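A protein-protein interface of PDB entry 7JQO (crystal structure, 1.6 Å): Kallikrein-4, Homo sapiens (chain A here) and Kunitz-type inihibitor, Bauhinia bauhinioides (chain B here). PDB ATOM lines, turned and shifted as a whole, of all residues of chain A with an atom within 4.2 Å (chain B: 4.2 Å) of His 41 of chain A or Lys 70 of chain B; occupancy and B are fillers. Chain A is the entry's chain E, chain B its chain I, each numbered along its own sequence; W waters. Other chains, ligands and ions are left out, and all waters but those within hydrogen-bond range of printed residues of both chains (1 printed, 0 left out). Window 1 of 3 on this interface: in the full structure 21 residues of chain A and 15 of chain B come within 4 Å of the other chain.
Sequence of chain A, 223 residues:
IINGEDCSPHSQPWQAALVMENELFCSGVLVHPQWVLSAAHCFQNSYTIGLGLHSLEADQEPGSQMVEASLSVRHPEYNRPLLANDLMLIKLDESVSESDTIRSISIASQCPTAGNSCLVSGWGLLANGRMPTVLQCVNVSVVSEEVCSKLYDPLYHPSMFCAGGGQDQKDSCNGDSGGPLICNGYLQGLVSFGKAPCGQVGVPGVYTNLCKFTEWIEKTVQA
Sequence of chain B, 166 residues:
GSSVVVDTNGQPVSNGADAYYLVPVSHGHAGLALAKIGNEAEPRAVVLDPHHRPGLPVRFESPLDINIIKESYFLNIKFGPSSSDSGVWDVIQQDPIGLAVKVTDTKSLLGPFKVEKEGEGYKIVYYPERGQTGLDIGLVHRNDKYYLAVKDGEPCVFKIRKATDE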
ATOM      1  N   ALA A  39      15.661  14.318  29.438  1.00  0.00           N
ATOM      2  CA  ALA A  39      15.169  14.921  28.194  1.00  0.00           C
ATOM      3  C   ALA A  39      13.803  14.326  27.858  1.00  0.00           C
ATOM      4  O   ALA A  39      13.611  13.123  28.024  1.00  0.00           O
ATOM      5  CB  ALA A  39      16.155  14.672  27.058  1.00  0.00           C
ATOM      6  N   ALA A  40      12.864  15.139  27.363  1.00  0.00           N
ATOM      7  CA  ALA A  40      11.545  14.628  26.993  1.00  0.00           C
ATOM      8  C   ALA A  40      11.656  13.633  25.832  1.00  0.00           C
ATOM      9  O   ALA A  40      10.805  12.758  25.680  1.00  0.00           O
ATOM     10  CB  ALA A  40      10.635  15.766  26.573  1.00  0.00           C
ATOM     11  N   HIS A  41      12.718  13.744  25.006  1.00  0.00           N
ATOM     12  CA  HIS A  41      12.837  12.792  23.903  1.00  0.00           C
ATOM     13  C   HIS A  41      13.193  11.376  24.377  1.00  0.00           C
ATOM     14  O   HIS A  41      13.088  10.428  23.572  1.00  0.00           O
ATOM     15  CB  HIS A  41      13.800  13.291  22.788  1.00  0.00           C
ATOM     16  CG  HIS A  41      15.256  13.238  23.153  1.00  0.00           C
ATOM     17  ND1 HIS A  41      15.962  14.370  23.612  1.00  0.00           N
ATOM     18  CD2 HIS A  41      16.165  12.231  23.073  1.00  0.00           C
ATOM     19  CE1 HIS A  41      17.239  14.056  23.810  1.00  0.00           C
ATOM     20  NE2 HIS A  41      17.399  12.739  23.490  1.00  0.00           N
ATOM     21  N   CYS A  42      13.526  11.242  25.674  1.00  0.00           N
ATOM     22  CA  CYS A  42      13.817   9.948  26.294  1.00  0.00           C
ATOM     23  C   CYS A  42      12.556   9.281  26.871  1.00  0.00           C
ATOM     24  O   CYS A  42      12.645   8.210  27.483  1.00  0.00           O
ATOM     25  CB  CYS A  42      14.887  10.047  27.384  1.00  0.00           C
ATOM     26  SG  CYS A  42      16.477  10.655  26.751  1.00  0.00           S
ATOM     27  N   PHE A  43      11.381   9.883  26.680  1.00  0.00           N
ATOM     28  CA  PHE A  43      10.124   9.411  27.285  1.00  0.00           C
ATOM     29  C   PHE A  43       9.866   7.941  26.947  1.00  0.00           C
ATOM     30  O   PHE A  43       9.985   7.524  25.789  1.00  0.00           O
ATOM     31  CB  PHE A  43       8.930  10.259  26.807  1.00  0.00           C
ATOM     32  CG  PHE A  43       7.602   9.715  27.272  1.00  0.00           C
ATOM     33  CD1 PHE A  43       7.109  10.053  28.524  1.00  0.00           C
ATOM     34  CD2 PHE A  43       6.869   8.828  26.483  1.00  0.00           C
ATOM     35  CE1 PHE A  43       5.889   9.548  28.977  1.00  0.00           C
ATOM     36  CE2 PHE A  43       5.664   8.301  26.941  1.00  0.00           C
ATOM     37  CZ  PHE A  43       5.178   8.657  28.195  1.00  0.00           C
ATOM     38  N   GLN A  44       9.458   7.183  27.978  1.00  0.00           N
ATOM     39  CA  GLN A  44       8.949   5.819  27.825  1.00  0.00           C
ATOM     40  C   GLN A  44       7.767   5.683  28.777  1.00  0.00           C
ATOM     41  O   GLN A  44       7.663   6.451  29.720  1.00  0.00           O
ATOM     42  CB  GLN A  44      10.048   4.803  28.194  1.00  0.00           C
ATOM     43  CG  GLN A  44      11.194   4.712  27.156  1.00  0.00           C
ATOM     44  CD  GLN A  44      10.729   4.034  25.877  1.00  0.00           C
ATOM     45  OE1 GLN A  44      10.744   2.796  25.743  1.00  0.00           O
ATOM     46  NE2 GLN A  44      10.337   4.818  24.882  1.00  0.00           N
ATOM     47  N   TYR A  78       6.903  20.652  24.803  1.00  0.00           N
ATOM     48  CA  TYR A  78       7.947  19.862  24.155  1.00  0.00           C
ATOM     49  C   TYR A  78       7.682  19.758  22.647  1.00  0.00           C
ATOM     50  O   TYR A  78       6.562  19.395  22.207  1.00  0.00           O
ATOM     51  CB  TYR A  78       8.017  18.480  24.814  1.00  0.00           C
ATOM     52  CG  TYR A  78       8.891  17.531  24.039  1.00  0.00           C
ATOM     53  CD1 TYR A  78      10.204  17.887  23.689  1.00  0.00           C
ATOM     54  CD2 TYR A  78       8.386  16.308  23.611  1.00  0.00           C
ATOM     55  CE1 TYR A  78      11.011  17.022  22.959  1.00  0.00           C
ATOM     56  CE2 TYR A  78       9.168  15.446  22.873  1.00  0.00           C
ATOM     57  CZ  TYR A  78      10.468  15.808  22.534  1.00  0.00           C
ATOM     58  OH  TYR A  78      11.204  14.944  21.795  1.00  0.00           O
ATOM     59  N   ASP A  86      12.857  20.598  25.796  1.00  0.00           N
ATOM     60  CA  ASP A  86      13.222  19.179  25.818  1.00  0.00           C
ATOM     61  C   ASP A  86      13.518  18.746  27.263  1.00  0.00           C
ATOM     62  O   ASP A  86      14.690  18.518  27.653  1.00  0.00           O
ATOM     63  CB  ASP A  86      14.395  18.897  24.860  1.00  0.00           C
ATOM     64  CG  ASP A  86      14.677  17.398  24.666  1.00  0.00           C
ATOM     65  OD1 ASP A  86      13.834  16.555  25.122  1.00  0.00           O
ATOM     66  OD2 ASP A  86      15.678  17.064  24.000  1.00  0.00           O
ATOM     67  N   SER A 177      22.269  11.842  26.024  1.00  0.00           N
ATOM     68  CA  SER A 177      20.973  12.533  26.159  1.00  0.00           C
ATOM     69  C   SER A 177      20.420  12.455  27.584  1.00  0.00           C
ATOM     70  O   SER A 177      20.393  11.350  28.182  1.00  0.00           O
ATOM     71  CB  SER A 177      19.878  11.908  25.225  1.00  0.00           C
ATOM     72  OG  SER A 177      20.012  12.531  23.968  1.00  0.00           O
ATOM     73  N   SER A 192      20.915  17.508  25.010  1.00  0.00           N
ATOM     74  CA  SER A 192      19.714  17.435  24.172  1.00  0.00           C
ATOM     75  C   SER A 192      20.047  16.952  22.749  1.00  0.00           C
ATOM     76  O   SER A 192      19.662  15.834  22.366  1.00  0.00           O
ATOM     77  CB  SER A 192      18.954  18.779  24.181  1.00  0.00           C
ATOM     78  OG  SER A 192      17.754  18.686  23.382  1.00  0.00           O
ATOM     79  N   GLY B   1       3.846   6.301  19.135  1.00  0.00           N
ATOM     80  CA  GLY B   1       5.030   7.107  18.727  1.00  0.00           C
ATOM     81  C   GLY B   1       6.203   6.918  19.692  1.00  0.00           C
ATOM     82  O   GLY B   1       7.362   7.027  19.269  1.00  0.00           O
ATOM     83  N   SER B   2       5.906   6.599  20.975  1.00  0.00           N
ATOM     84  CA  SER B   2       6.942   6.452  22.001  1.00  0.00           C
ATOM     85  C   SER B   2       7.618   5.084  21.862  1.00  0.00           C
ATOM     86  O   SER B   2       8.614   4.736  22.542  1.00  0.00           O
ATOM     87  CB  SER B   2       6.388   6.647  23.388  1.00  0.00           C
ATOM     88  OG  SER B   2       5.988   5.398  23.947  1.00  0.00           O
ATOM     89  N   SER B   3       7.010   4.295  20.983  1.00  0.00           N
ATOM     90  CA  SER B   3       7.569   3.018  20.596  1.00  0.00           C
ATOM     91  C   SER B   3       8.945   3.198  19.975  1.00  0.00           C
ATOM     92  O   SER B   3       9.170   4.022  19.076  1.00  0.00           O
ATOM     93  CB  SER B   3       6.684   2.306  19.657  1.00  0.00           C
ATOM     94  OG  SER B   3       5.563   1.820  20.367  1.00  0.00           O
ATOM     95  N   VAL B   5      11.762   1.819  17.574  1.00  0.00           N
ATOM     96  CA  VAL B   5      11.851   1.022  16.354  1.00  0.00           C
ATOM     97  C   VAL B   5      12.838  -0.116  16.596  1.00  0.00           C
ATOM     98  O   VAL B   5      13.963   0.142  17.027  1.00  0.00           O
ATOM     99  CB  VAL B   5      12.313   1.875  15.157  1.00  0.00           C
ATOM    100  CG1 VAL B   5      12.482   1.036  13.879  1.00  0.00           C
ATOM    101  CG2 VAL B   5      11.374   3.072  14.933  1.00  0.00           C
ATOM    102  N   LEU B  64      19.233  14.162  17.911  1.00  0.00           N
ATOM    103  CA  LEU B  64      19.129  13.916  19.346  1.00  0.00           C
ATOM    104  C   LEU B  64      20.307  13.053  19.816  1.00  0.00           C
ATOM    105  O   LEU B  64      20.724  12.126  19.106  1.00  0.00           O
ATOM    106  CB  LEU B  64      17.812  13.182  19.645  1.00  0.00           C
ATOM    107  CG  LEU B  64      16.522  13.951  19.254  1.00  0.00           C
ATOM    108  CD1 LEU B  64      15.300  13.032  19.368  1.00  0.00           C
ATOM    109  CD2 LEU B  64      16.339  15.215  20.129  1.00  0.00           C
ATOM    110  N   ILE B  66      20.718  10.552  21.548  1.00  0.00           N
ATOM    111  CA  ILE B  66      20.265   9.241  21.996  1.00  0.00           C
ATOM    112  C   ILE B  66      20.752   8.211  20.979  1.00  0.00           C
ATOM    113  O   ILE B  66      21.011   8.560  19.820  1.00  0.00           O
ATOM    114  CB  ILE B  66      18.725   9.263  22.157  1.00  0.00           C
ATOM    115  CG1 ILE B  66      18.191   8.009  22.876  1.00  0.00           C
ATOM    116  CG2 ILE B  66      18.016   9.512  20.812  1.00  0.00           C
ATOM    117  CD1 ILE B  66      16.736   8.130  23.265  1.00  0.00           C
ATOM    118  N   ILE B  69      16.210   4.857  18.033  1.00  0.00           N
ATOM    119  CA  ILE B  69      15.248   5.617  17.234  1.00  0.00           C
ATOM    120  C   ILE B  69      13.834   5.265  17.704  1.00  0.00           C
ATOM    121  O   ILE B  69      13.517   4.073  17.863  1.00  0.00           O
ATOM    122  CB  ILE B  69      15.445   5.246  15.738  1.00  0.00           C
ATOM    123  CG1 ILE B  69      16.846   5.659  15.268  1.00  0.00           C
ATOM    124  CG2 ILE B  69      14.324   5.786  14.872  1.00  0.00           C
ATOM    125  CD1 ILE B  69      17.120   7.118  15.399  1.00  0.00           C
ATOM    126  N   LYS B  70      13.000   6.296  17.922  1.00  0.00           N
ATOM    127  CA  LYS B  70      11.579   6.139  18.203  1.00  0.00           C
ATOM    128  C   LYS B  70      10.763   6.443  16.946  1.00  0.00           C
ATOM    129  O   LYS B  70      11.193   7.214  16.069  1.00  0.00           O
ATOM    130  CB  LYS B  70      11.132   7.060  19.348  1.00  0.00           C
ATOM    131  CG  LYS B  70      11.646   6.682  20.741  1.00  0.00           C
ATOM    132  CD  LYS B  70      11.116   7.837  21.606  1.00  0.00           C
ATOM    133  CE  LYS B  70      11.115   7.779  23.082  1.00  0.00           C
ATOM    134  NZ  LYS B  70      10.302   8.958  23.428  1.00  0.00           N
ATOM    135  N   GLU B  71       9.539   5.886  16.888  1.00  0.00           N
ATOM    136  CA  GLU B  71       8.653   6.115  15.745  1.00  0.00           C
ATOM    137  C   GLU B  71       8.281   7.593  15.608  1.00  0.00           C
ATOM    138  O   GLU B  71       7.927   8.046  14.518  1.00  0.00           O
ATOM    139  CB  GLU B  71       7.386   5.244  15.882  1.00  0.00           C
ATOM    140  CG  GLU B  71       7.692   3.761  15.781  1.00  0.00           C
ATOM    141  CD  GLU B  71       6.431   2.918  15.856  1.00  0.00           C
ATOM    142  OE1 GLU B  71       5.378   3.399  15.332  1.00  0.00           O
ATOM    143  OE2 GLU B  71       6.479   1.809  16.471  1.00  0.00           O
ATOM    144  N   SER B  72       8.348   8.359  16.697  1.00  0.00           N
ATOM    145  CA  SER B  72       7.974   9.775  16.657  1.00  0.00           C
ATOM    146  C   SER B  72       9.083  10.698  16.155  1.00  0.00           C
ATOM    147  O   SER B  72       8.815  11.884  15.917  1.00  0.00           O
ATOM    148  CB  SER B  72       7.512  10.257  18.023  1.00  0.00           C
ATOM    149  OG  SER B  72       8.535  10.031  18.989  1.00  0.00           O
ATOM    150  N   TYR B  73      10.316  10.201  16.036  1.00  0.00           N
ATOM    151  CA  TYR B  73      11.421  11.083  15.668  1.00  0.00           C
ATOM    152  C   TYR B  73      11.415  11.403  14.179  1.00  0.00           C
ATOM    153  O   TYR B  73      11.271  10.519  13.343  1.00  0.00           O
ATOM    154  CB  TYR B  73      12.768  10.413  15.948  1.00  0.00           C
ATOM    155  CG  TYR B  73      13.130  10.189  17.401  1.00  0.00           C
ATOM    156  CD1 TYR B  73      12.394  10.738  18.459  1.00  0.00           C
ATOM    157  CD2 TYR B  73      14.280   9.452  17.706  1.00  0.00           C
ATOM    158  CE1 TYR B  73      12.797  10.541  19.786  1.00  0.00           C
ATOM    159  CE2 TYR B  73      14.696   9.255  19.022  1.00  0.00           C
ATOM    160  CZ  TYR B  73      13.948   9.804  20.060  1.00  0.00           C
ATOM    161  OH  TYR B  73      14.367   9.592  21.338  1.00  0.00           O
HETATM  162  O   HOH W   1       9.205  11.731  23.611  1.00  0.00           O
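N of Ile 66 of chain B is in hydrogen-bond range of OG of Ser 177 of chain A (3.2 Å). The side-chain amino group (NZ) of Lys 70 of chain B is in hydrogen-bond range of the backbone carbonyl oxygen (O) of His 41 of chain A (3.2 Å). O of His 41 of chain A is in hydrogen-bond range of OH of Tyr 73 of chain B, 2.7 Å away. The backbone carbonyl oxygen of Phe 43 of chain A is in hydrogen-bond range of the side-chain amino group of Lys 70 of chain B, at 2.8 Å. The backbone carbonyl oxygen of Ser 2 of chain B lies within hydrogen-bond range of the side-chain amide nitrogen of Gln 44 of chain A (2.9 Å).
NE2 of His 41 of chain A lies within hydrogen-bond range of OG of Ser 177 of chain A (2.7 Å). OD2 of Asp 86 of chain A is in hydrogen-bond range of ND1 of His 41 of chain A. The side-chain carboxylate (OD2) of Asp 86 of chain A sits at hydrogen-bond distance from the side-chain hydroxyl (OG) of Ser 192 of chain A (2.7 Å).
ND1 of His 41 of chain A touches CD2 of Leu 64 of chain B (3.6 Å). His 41 of chain A touches Ile 66 of chain B. Phe 43 of chain A touches Ser 2 of chain B (CD2 to CB, 3.8 Å). Gln 44 of chain A touches Lys 70 of chain B. Ser 192 of chain A touches Leu 64 of chain B.
Printed residues of chain B within 4 Å of Phe 43 of chain A: Ser 2 (3.8 Å) and Lys 70 (2.8 Å). Tyr 78 of chain A touches none of the printed residues of chain B. Printed residues of chain B within 4 Å of Ser 192 of chain A: Leu 64 (3.6 Å). Of the printed residues of chain A, Ser 2 of chain B touches Phe 43 (3.8 Å) and Gln 44 (2.9 Å). Lys 70 of chain B touches three residues of chain A. The nearest printed residue of chain A that does not touch Leu 64 of chain B is Ser 177 of chain A (4.2 Å).
Of the 11 printed residues of chain B, 5 touch a printed residue of chain A. Hydrophobic or aromatic side chains of chain B within 4 Å of the printed part of chain A: Leu 64, Ile 66 and Tyr 73. Hydrophobic or aromatic side chains of chain A within 4 Å of the printed part of chain B: His 41 and Phe 43. Along chain A the printed residues that touch a printed residue of chain B span positions 41 to 192. Among the printed residues, no Asp or Glu carboxylate lies within 4 Å of a Lys or Arg side-chain nitrogen of the other chain.
Water W1 lies within hydrogen-bond range of the backbone carbonyl oxygen (O) of Ala 40 of chain A (2.8 Å) and the side-chain amino group (NZ) of Lys 70 of chain B (3.0 Å).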
